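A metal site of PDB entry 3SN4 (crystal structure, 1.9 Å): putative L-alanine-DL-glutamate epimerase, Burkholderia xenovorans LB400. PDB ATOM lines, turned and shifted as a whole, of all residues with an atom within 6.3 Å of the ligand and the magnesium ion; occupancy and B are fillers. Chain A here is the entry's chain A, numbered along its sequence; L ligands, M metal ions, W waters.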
ATOM      1  N   PHE A  41     -17.584 -25.040  -3.088  1.00  0.00           N
ATOM      2  CA  PHE A  41     -17.000 -23.705  -2.901  1.00  0.00           C
ATOM      3  C   PHE A  41     -15.516 -23.730  -3.213  1.00  0.00           C
ATOM      4  O   PHE A  41     -14.649 -23.616  -2.331  1.00  0.00           O
ATOM      5  CB  PHE A  41     -17.269 -23.171  -1.505  1.00  0.00           C
ATOM      6  CG  PHE A  41     -17.031 -21.678  -1.358  1.00  0.00           C
ATOM      7  CD1 PHE A  41     -17.538 -20.778  -2.302  1.00  0.00           C
ATOM      8  CD2 PHE A  41     -16.332 -21.163  -0.280  1.00  0.00           C
ATOM      9  CE1 PHE A  41     -17.340 -19.415  -2.167  1.00  0.00           C
ATOM     10  CE2 PHE A  41     -16.135 -19.778  -0.140  1.00  0.00           C
ATOM     11  CZ  PHE A  41     -16.626 -18.917  -1.098  1.00  0.00           C
ATOM     12  N   TYR A 122     -27.616 -13.211  11.415  1.00  0.00           N
ATOM     13  CA  TYR A 122     -28.164 -12.536  10.253  1.00  0.00           C
ATOM     14  C   TYR A 122     -28.611 -13.550   9.201  1.00  0.00           C
ATOM     15  O   TYR A 122     -28.026 -14.618   9.060  1.00  0.00           O
ATOM     16  CB  TYR A 122     -27.181 -11.545   9.643  1.00  0.00           C
ATOM     17  CG  TYR A 122     -25.937 -12.108   9.047  1.00  0.00           C
ATOM     18  CD1 TYR A 122     -25.835 -12.339   7.674  1.00  0.00           C
ATOM     19  CD2 TYR A 122     -24.810 -12.343   9.841  1.00  0.00           C
ATOM     20  CE1 TYR A 122     -24.638 -12.815   7.103  1.00  0.00           C
ATOM     21  CE2 TYR A 122     -23.621 -12.830   9.276  1.00  0.00           C
ATOM     22  CZ  TYR A 122     -23.546 -13.041   7.919  1.00  0.00           C
ATOM     23  OH  TYR A 122     -22.390 -13.507   7.402  1.00  0.00           O
ATOM     24  N   SER A 124     -28.550 -14.664   5.832  1.00  0.00           N
ATOM     25  CA  SER A 124     -27.553 -14.489   4.800  1.00  0.00           C
ATOM     26  C   SER A 124     -28.122 -14.857   3.465  1.00  0.00           C
ATOM     27  O   SER A 124     -29.170 -15.506   3.383  1.00  0.00           O
ATOM     28  CB  SER A 124     -26.336 -15.357   5.099  1.00  0.00           C
ATOM     29  OG  SER A 124     -25.311 -14.984   4.220  1.00  0.00           O
ATOM     30  N   HIS A 125     -27.423 -14.399   2.406  1.00  0.00           N
ATOM     31  CA  HIS A 125     -27.856 -14.599   1.016  1.00  0.00           C
ATOM     32  C   HIS A 125     -29.322 -14.202   0.835  1.00  0.00           C
ATOM     33  O   HIS A 125     -30.128 -14.965   0.291  1.00  0.00           O
ATOM     34  CB  HIS A 125     -27.639 -16.060   0.602  1.00  0.00           C
ATOM     35  CG  HIS A 125     -26.201 -16.450   0.655  1.00  0.00           C
ATOM     36  ND1 HIS A 125     -25.654 -17.121   1.720  1.00  0.00           N
ATOM     37  CD2 HIS A 125     -25.190 -16.188  -0.200  1.00  0.00           C
ATOM     38  CE1 HIS A 125     -24.360 -17.290   1.503  1.00  0.00           C
ATOM     39  NE2 HIS A 125     -24.053 -16.731   0.341  1.00  0.00           N
ATOM     40  N   THR A 128     -30.142 -13.069  -2.180  1.00  0.00           N
ATOM     41  CA  THR A 128     -29.252 -13.777  -3.086  1.00  0.00           C
ATOM     42  C   THR A 128     -29.727 -15.174  -3.520  1.00  0.00           C
ATOM     43  O   THR A 128     -29.701 -15.488  -4.711  1.00  0.00           O
ATOM     44  CB  THR A 128     -27.833 -13.868  -2.482  1.00  0.00           C
ATOM     45  OG1 THR A 128     -27.474 -12.560  -1.978  1.00  0.00           O
ATOM     46  CG2 THR A 128     -26.825 -14.373  -3.537  1.00  0.00           C
ATOM     47  N   TRP A 129     -30.147 -15.996  -2.567  1.00  0.00           N
ATOM     48  CA  TRP A 129     -30.591 -17.360  -2.886  1.00  0.00           C
ATOM     49  C   TRP A 129     -31.865 -17.341  -3.759  1.00  0.00           C
ATOM     50  O   TRP A 129     -32.007 -18.146  -4.710  1.00  0.00           O
ATOM     51  CB  TRP A 129     -30.853 -18.132  -1.584  1.00  0.00           C
ATOM     52  CG  TRP A 129     -29.655 -18.914  -0.946  1.00  0.00           C
ATOM     53  CD1 TRP A 129     -29.750 -19.757   0.148  1.00  0.00           C
ATOM     54  CD2 TRP A 129     -28.273 -18.944  -1.349  1.00  0.00           C
ATOM     55  NE1 TRP A 129     -28.525 -20.295   0.451  1.00  0.00           N
ATOM     56  CE2 TRP A 129     -27.598 -19.809  -0.436  1.00  0.00           C
ATOM     57  CE3 TRP A 129     -27.535 -18.322  -2.357  1.00  0.00           C
ATOM     58  CZ2 TRP A 129     -26.228 -20.062  -0.515  1.00  0.00           C
ATOM     59  CZ3 TRP A 129     -26.173 -18.570  -2.438  1.00  0.00           C
ATOM     60  CH2 TRP A 129     -25.525 -19.438  -1.514  1.00  0.00           C
ATOM     61  N   LYS A 163     -28.006 -10.107   4.811  1.00  0.00           N
ATOM     62  CA  LYS A 163     -26.821  -9.911   3.958  1.00  0.00           C
ATOM     63  C   LYS A 163     -27.127 -10.198   2.505  1.00  0.00           C
ATOM     64  O   LYS A 163     -27.642 -11.270   2.175  1.00  0.00           O
ATOM     65  CB  LYS A 163     -25.639 -10.786   4.406  1.00  0.00           C
ATOM     66  CG  LYS A 163     -24.319 -10.351   3.763  1.00  0.00           C
ATOM     67  CD  LYS A 163     -23.074 -10.977   4.399  1.00  0.00           C
ATOM     68  CE  LYS A 163     -22.823 -12.399   3.876  1.00  0.00           C
ATOM     69  NZ  LYS A 163     -21.802 -13.138   4.689  1.00  0.00           N
ATOM     70  N   ASN A 165     -25.626  -9.543  -1.817  1.00  0.00           N
ATOM     71  CA  ASN A 165     -24.428  -9.560  -2.661  1.00  0.00           C
ATOM     72  C   ASN A 165     -24.585  -8.537  -3.791  1.00  0.00           C
ATOM     73  O   ASN A 165     -25.219  -7.523  -3.571  1.00  0.00           O
ATOM     74  CB  ASN A 165     -24.164 -10.979  -3.179  1.00  0.00           C
ATOM     75  CG  ASN A 165     -24.042 -11.966  -2.064  1.00  0.00           C
ATOM     76  OD1 ASN A 165     -25.058 -12.417  -1.504  1.00  0.00           O
ATOM     77  ND2 ASN A 165     -22.813 -12.350  -1.736  1.00  0.00           N
ATOM     78  N   ARG A 178     -20.603 -11.811 -10.391  1.00  0.00           N
ATOM     79  CA  ARG A 178     -19.652 -12.647  -9.634  1.00  0.00           C
ATOM     80  C   ARG A 178     -18.363 -12.927 -10.421  1.00  0.00           C
ATOM     81  O   ARG A 178     -17.939 -14.078 -10.539  1.00  0.00           O
ATOM     82  CB  ARG A 178     -20.315 -13.978  -9.263  1.00  0.00           C
ATOM     83  CG  ARG A 178     -21.387 -13.831  -8.194  1.00  0.00           C
ATOM     84  CD  ARG A 178     -22.407 -14.947  -8.222  1.00  0.00           C
ATOM     85  NE  ARG A 178     -21.829 -16.284  -8.080  1.00  0.00           N
ATOM     86  CZ  ARG A 178     -21.343 -16.796  -6.946  1.00  0.00           C
ATOM     87  NH1 ARG A 178     -20.857 -18.040  -6.945  1.00  0.00           N
ATOM     88  NH2 ARG A 178     -21.330 -16.077  -5.799  1.00  0.00           N
ATOM     89  N   PHE A 181     -15.512 -15.199  -9.389  1.00  0.00           N
ATOM     90  CA  PHE A 181     -15.743 -16.624  -9.593  1.00  0.00           C
ATOM     91  C   PHE A 181     -16.059 -16.956 -11.070  1.00  0.00           C
ATOM     92  O   PHE A 181     -16.658 -17.993 -11.411  1.00  0.00           O
ATOM     93  CB  PHE A 181     -16.880 -17.084  -8.654  1.00  0.00           C
ATOM     94  CG  PHE A 181     -16.623 -16.868  -7.170  1.00  0.00           C
ATOM     95  CD1 PHE A 181     -15.348 -17.019  -6.620  1.00  0.00           C
ATOM     96  CD2 PHE A 181     -17.693 -16.607  -6.291  1.00  0.00           C
ATOM     97  CE1 PHE A 181     -15.113 -16.862  -5.255  1.00  0.00           C
ATOM     98  CE2 PHE A 181     -17.475 -16.455  -4.922  1.00  0.00           C
ATOM     99  CZ  PHE A 181     -16.177 -16.575  -4.389  1.00  0.00           C
ATOM    100  N   ASP A 219     -21.864  -8.241   1.032  1.00  0.00           N
ATOM    101  CA  ASP A 219     -20.728  -9.103   0.719  1.00  0.00           C
ATOM    102  C   ASP A 219     -20.327  -8.883  -0.728  1.00  0.00           C
ATOM    103  O   ASP A 219     -21.140  -9.057  -1.648  1.00  0.00           O
ATOM    104  CB  ASP A 219     -21.076 -10.562   0.975  1.00  0.00           C
ATOM    105  CG  ASP A 219     -19.852 -11.487   1.025  1.00  0.00           C
ATOM    106  OD1 ASP A 219     -18.739 -11.132   0.574  1.00  0.00           O
ATOM    107  OD2 ASP A 219     -20.044 -12.621   1.520  1.00  0.00           O
ATOM    108  N   ASN A 221     -17.336 -10.374  -1.743  1.00  0.00           N
ATOM    109  CA  ASN A 221     -16.559 -11.600  -2.005  1.00  0.00           C
ATOM    110  C   ASN A 221     -15.209 -11.231  -2.641  1.00  0.00           C
ATOM    111  O   ASN A 221     -14.563 -10.301  -2.158  1.00  0.00           O
ATOM    112  CB  ASN A 221     -17.358 -12.598  -2.861  1.00  0.00           C
ATOM    113  CG  ASN A 221     -18.634 -13.067  -2.190  1.00  0.00           C
ATOM    114  OD1 ASN A 221     -19.709 -12.552  -2.478  1.00  0.00           O
ATOM    115  ND2 ASN A 221     -18.509 -14.054  -1.312  1.00  0.00           N
ATOM    116  N   GLU A 245     -18.122  -6.881   3.355  1.00  0.00           N
ATOM    117  CA  GLU A 245     -17.318  -8.075   3.392  1.00  0.00           C
ATOM    118  C   GLU A 245     -16.538  -8.152   2.107  1.00  0.00           C
ATOM    119  O   GLU A 245     -17.095  -8.041   1.017  1.00  0.00           O
ATOM    120  CB  GLU A 245     -18.242  -9.266   3.542  1.00  0.00           C
ATOM    121  CG  GLU A 245     -17.616 -10.596   3.929  1.00  0.00           C
ATOM    122  CD  GLU A 245     -18.695 -11.621   4.335  1.00  0.00           C
ATOM    123  OE1 GLU A 245     -18.479 -12.811   4.135  1.00  0.00           O
ATOM    124  OE2 GLU A 245     -19.775 -11.211   4.834  1.00  0.00           O
ATOM    125  N   ASP A 247     -13.196 -10.340   0.424  1.00  0.00           N
ATOM    126  CA  ASP A 247     -12.140 -11.330   0.465  1.00  0.00           C
ATOM    127  C   ASP A 247     -10.950 -10.931  -0.394  1.00  0.00           C
ATOM    128  O   ASP A 247     -11.124 -10.472  -1.529  1.00  0.00           O
ATOM    129  CB  ASP A 247     -12.657 -12.680   0.027  1.00  0.00           C
ATOM    130  CG  ASP A 247     -13.758 -13.181   0.904  1.00  0.00           C
ATOM    131  OD1 ASP A 247     -13.564 -13.274   2.142  1.00  0.00           O
ATOM    132  OD2 ASP A 247     -14.815 -13.466   0.328  1.00  0.00           O
ATOM    133  N   GLU A 269     -12.861 -15.330   5.510  1.00  0.00           N
ATOM    134  CA  GLU A 269     -13.634 -16.575   5.517  1.00  0.00           C
ATOM    135  C   GLU A 269     -12.933 -17.736   4.842  1.00  0.00           C
ATOM    136  O   GLU A 269     -13.289 -18.908   5.053  1.00  0.00           O
ATOM    137  CB  GLU A 269     -15.028 -16.376   4.882  1.00  0.00           C
ATOM    138  CG  GLU A 269     -15.055 -16.344   3.351  1.00  0.00           C
ATOM    139  CD  GLU A 269     -16.396 -15.946   2.748  1.00  0.00           C
ATOM    140  OE1 GLU A 269     -16.651 -16.326   1.574  1.00  0.00           O
ATOM    141  OE2 GLU A 269     -17.217 -15.262   3.422  1.00  0.00           O
ATOM    142  N   ILE A 290     -14.037 -13.205   9.853  1.00  0.00           N
ATOM    143  CA  ILE A 290     -14.945 -14.322   9.570  1.00  0.00           C
ATOM    144  C   ILE A 290     -14.104 -15.583   9.636  1.00  0.00           C
ATOM    145  O   ILE A 290     -13.048 -15.658   9.022  1.00  0.00           O
ATOM    146  CB  ILE A 290     -15.642 -14.139   8.220  1.00  0.00           C
ATOM    147  CG1 ILE A 290     -16.558 -12.891   8.309  1.00  0.00           C
ATOM    148  CG2 ILE A 290     -16.490 -15.384   7.853  1.00  0.00           C
ATOM    149  CD1 ILE A 290     -17.060 -12.342   6.960  1.00  0.00           C
ATOM    150  N   HIS A 318     -18.435 -18.539   9.459  1.00  0.00           N
ATOM    151  CA  HIS A 318     -18.896 -18.698   8.091  1.00  0.00           C
ATOM    152  C   HIS A 318     -19.814 -19.892   8.036  1.00  0.00           C
ATOM    153  O   HIS A 318     -19.381 -21.018   8.284  1.00  0.00           O
ATOM    154  CB  HIS A 318     -17.678 -18.951   7.210  1.00  0.00           C
ATOM    155  CG  HIS A 318     -17.954 -18.796   5.751  1.00  0.00           C
ATOM    156  ND1 HIS A 318     -17.172 -19.405   4.799  1.00  0.00           N
ATOM    157  CD2 HIS A 318     -18.932 -18.129   5.088  1.00  0.00           C
ATOM    158  CE1 HIS A 318     -17.628 -19.084   3.598  1.00  0.00           C
ATOM    159  NE2 HIS A 318     -18.712 -18.328   3.753  1.00  0.00           N
ATOM    160  N   ASN A 319     -21.071 -19.656   7.696  1.00  0.00           N
ATOM    161  CA  ASN A 319     -22.089 -20.690   7.785  1.00  0.00           C
ATOM    162  C   ASN A 319     -23.104 -20.516   6.680  1.00  0.00           C
ATOM    163  O   ASN A 319     -24.035 -19.694   6.806  1.00  0.00           O
ATOM    164  CB  ASN A 319     -22.781 -20.580   9.141  1.00  0.00           C
ATOM    165  CG  ASN A 319     -23.750 -21.692   9.391  1.00  0.00           C
ATOM    166  OD1 ASN A 319     -23.400 -22.872   9.262  1.00  0.00           O
ATOM    167  ND2 ASN A 319     -24.988 -21.338   9.757  1.00  0.00           N
ATOM    168  N   PHE A 320     -22.919 -21.263   5.585  1.00  0.00           N
ATOM    169  CA  PHE A 320     -23.845 -21.186   4.456  1.00  0.00           C
ATOM    170  C   PHE A 320     -24.091 -22.536   3.798  1.00  0.00           C
ATOM    171  O   PHE A 320     -24.282 -22.636   2.559  1.00  0.00           O
ATOM    172  CB  PHE A 320     -23.394 -20.122   3.429  1.00  0.00           C
ATOM    173  CG  PHE A 320     -22.249 -20.543   2.527  1.00  0.00           C
ATOM    174  CD1 PHE A 320     -22.439 -20.686   1.160  1.00  0.00           C
ATOM    175  CD2 PHE A 320     -20.972 -20.764   3.040  1.00  0.00           C
ATOM    176  CE1 PHE A 320     -21.383 -21.076   0.321  1.00  0.00           C
ATOM    177  CE2 PHE A 320     -19.922 -21.147   2.191  1.00  0.00           C
ATOM    178  CZ  PHE A 320     -20.131 -21.297   0.836  1.00  0.00           C
ATOM    179  N   GLU A 343     -23.793 -16.134  11.096  1.00  0.00           N
ATOM    180  CA  GLU A 343     -24.399 -16.224   9.769  1.00  0.00           C
ATOM    181  C   GLU A 343     -25.320 -17.419   9.724  1.00  0.00           C
ATOM    182  O   GLU A 343     -25.008 -18.481  10.227  1.00  0.00           O
ATOM    183  CB  GLU A 343     -23.325 -16.424   8.710  1.00  0.00           C
ATOM    184  CG  GLU A 343     -23.865 -16.519   7.285  1.00  0.00           C
ATOM    185  CD  GLU A 343     -22.773 -16.588   6.230  1.00  0.00           C
ATOM    186  OE1 GLU A 343     -21.625 -16.989   6.559  1.00  0.00           O
ATOM    187  OE2 GLU A 343     -23.074 -16.210   5.074  1.00  0.00           O
ATOM    188  N   ASP A 345     -28.310 -19.186   6.723  1.00  0.00           N
ATOM    189  CA  ASP A 345     -29.210 -19.134   5.565  1.00  0.00           C
ATOM    190  C   ASP A 345     -30.614 -19.541   6.011  1.00  0.00           C
ATOM    191  O   ASP A 345     -30.869 -20.681   6.395  1.00  0.00           O
ATOM    192  CB  ASP A 345     -28.723 -20.022   4.434  1.00  0.00           C
ATOM    193  CG  ASP A 345     -27.451 -19.490   3.733  1.00  0.00           C
ATOM    194  OD1 ASP A 345     -27.238 -18.247   3.617  1.00  0.00           O
ATOM    195  OD2 ASP A 345     -26.672 -20.343   3.232  1.00  0.00           O
ATOM    196  N   LEU A 395     -19.338 -23.348  -7.286  1.00  0.00           N
ATOM    197  CA  LEU A 395     -18.518 -22.547  -8.224  1.00  0.00           C
ATOM    198  C   LEU A 395     -18.168 -23.311  -9.482  1.00  0.00           C
ATOM    199  O   LEU A 395     -17.926 -22.704 -10.536  1.00  0.00           O
ATOM    200  CB  LEU A 395     -17.205 -22.082  -7.561  1.00  0.00           C
ATOM    201  CG  LEU A 395     -17.345 -21.325  -6.253  1.00  0.00           C
ATOM    202  CD1 LEU A 395     -15.985 -20.738  -5.860  1.00  0.00           C
ATOM    203  CD2 LEU A 395     -18.468 -20.246  -6.341  1.00  0.00           C
HETATM  204  C1  LIG L   1     -20.638 -16.053   2.665  1.00  0.00           C
HETATM  205  O1  LIG L   1     -21.464 -16.911   3.078  1.00  0.00           O
HETATM  206  O2  LIG L   1     -20.389 -15.003   3.352  1.00  0.00           O
HETATM  207  C2  LIG L   1     -19.904 -16.265   1.386  1.00  0.00           C
HETATM  208  O3  LIG L   1     -19.224 -15.361   0.900  1.00  0.00           O
HETATM  209  C3  LIG L   1     -19.870 -17.587   0.659  1.00  0.00           C
HETATM  210  C4  LIG L   1     -20.847 -17.827  -0.507  1.00  0.00           C
HETATM  211  C5  LIG L   1     -20.965 -16.848  -1.666  1.00  0.00           C
HETATM  212  O4  LIG L   1     -21.592 -15.786  -1.455  1.00  0.00           O
HETATM  213  O5  LIG L   1     -20.491 -17.165  -2.799  1.00  0.00           O
HETATM  214 MG    MG M   1     -18.637 -13.946   2.375  1.00  0.00          MG
HETATM  215  O   HOH W   1     -17.086 -13.075   1.372  1.00  0.00           O
HETATM  216  O   HOH W   2     -19.440 -14.627   6.176  1.00  0.00           O
HETATM  217  O   HOH W   3     -22.209 -13.927   0.647  1.00  0.00           O
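Residues that only touch the ligand: Phe 41, Asn 165, Phe 181 and Phe 320.
Hydrophobic or aromatic side chains within 4 Å of the ligand: Phe 41, His 125, Phe 181, His 318 and Phe 320.
The nearest printed residue that does not touch the ligand is Ser 124 (4.5 Å).
A ring nitrogen (NE2) of His 318 lies within hydrogen-bond range of an oxygen (O1) of the ligand (3.2 Å).
The side-chain amide nitrogen (ND2) of Asn 221 lies close to an oxygen (O3) of the ligand (2.7 Å).
The side-chain amino group (NZ) of Lys 163 lies close to an oxygen (O2) of the ligand, 2.7 Å away.
An oxygen (O1) of the ligand lies close to the side-chain carboxylate (OE2) of Glu 343 (2.7 Å).
NE2 of His 125 is in hydrogen-bond range of O4 of the ligand (3.2 Å).
An oxygen (O5) of the ligand is in salt-bridge range of the guanidinium group (NH2) of Arg 178, at 3.3 Å.
ND2 of Asn 221 touches the magnesium ion, 3.7 Å away.
Water W3 lies within hydrogen-bond range of an oxygen (O4) of the ligand, the side-chain amide nitrogen of Asn 165 and a ring nitrogen (NE2) of His 125.
Water W2 lies within hydrogen-bond range of NZ of Lys 163, OE1 of Glu 343 and OH of Tyr 122.
The side-chain carboxylate (OD2) of Asp 219 sits close to the side-chain amino group (NZ) of Lys 163.
The side-chain hydroxyl of Ser 124 sits at hydrogen-bond distance from the side-chain carboxylate of Glu 343 (2.7 Å).
The backbone NH (N) of Asp 247 lies within hydrogen-bond range of the backbone carbonyl oxygen (O) of Asn 221 (2.9 Å).
O of Lys 163 is in hydrogen-bond range of N of His 125 (3.1 Å).
NE2 of His 318 lies close to OE2 of Glu 269 (3.4 Å).
The side-chain amide nitrogen (ND2) of Asn 165 lies within hydrogen-bond range of the side-chain amide oxygen (OD1) of Asn 221, 3.2 Å away.
NZ of Lys 163 is in hydrogen-bond range of OH of Tyr 122, at 2.8 Å.
The side-chain amino group of Lys 163 lies within salt-bridge range of the side-chain carboxylate of Glu 245, at 2.8 Å.
The magnesium ion is bound by water W1, OE1 of Glu 245, OD2 of Asp 219, O3 of the ligand, OE2 of Glu 269 and O2 of the ligand.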
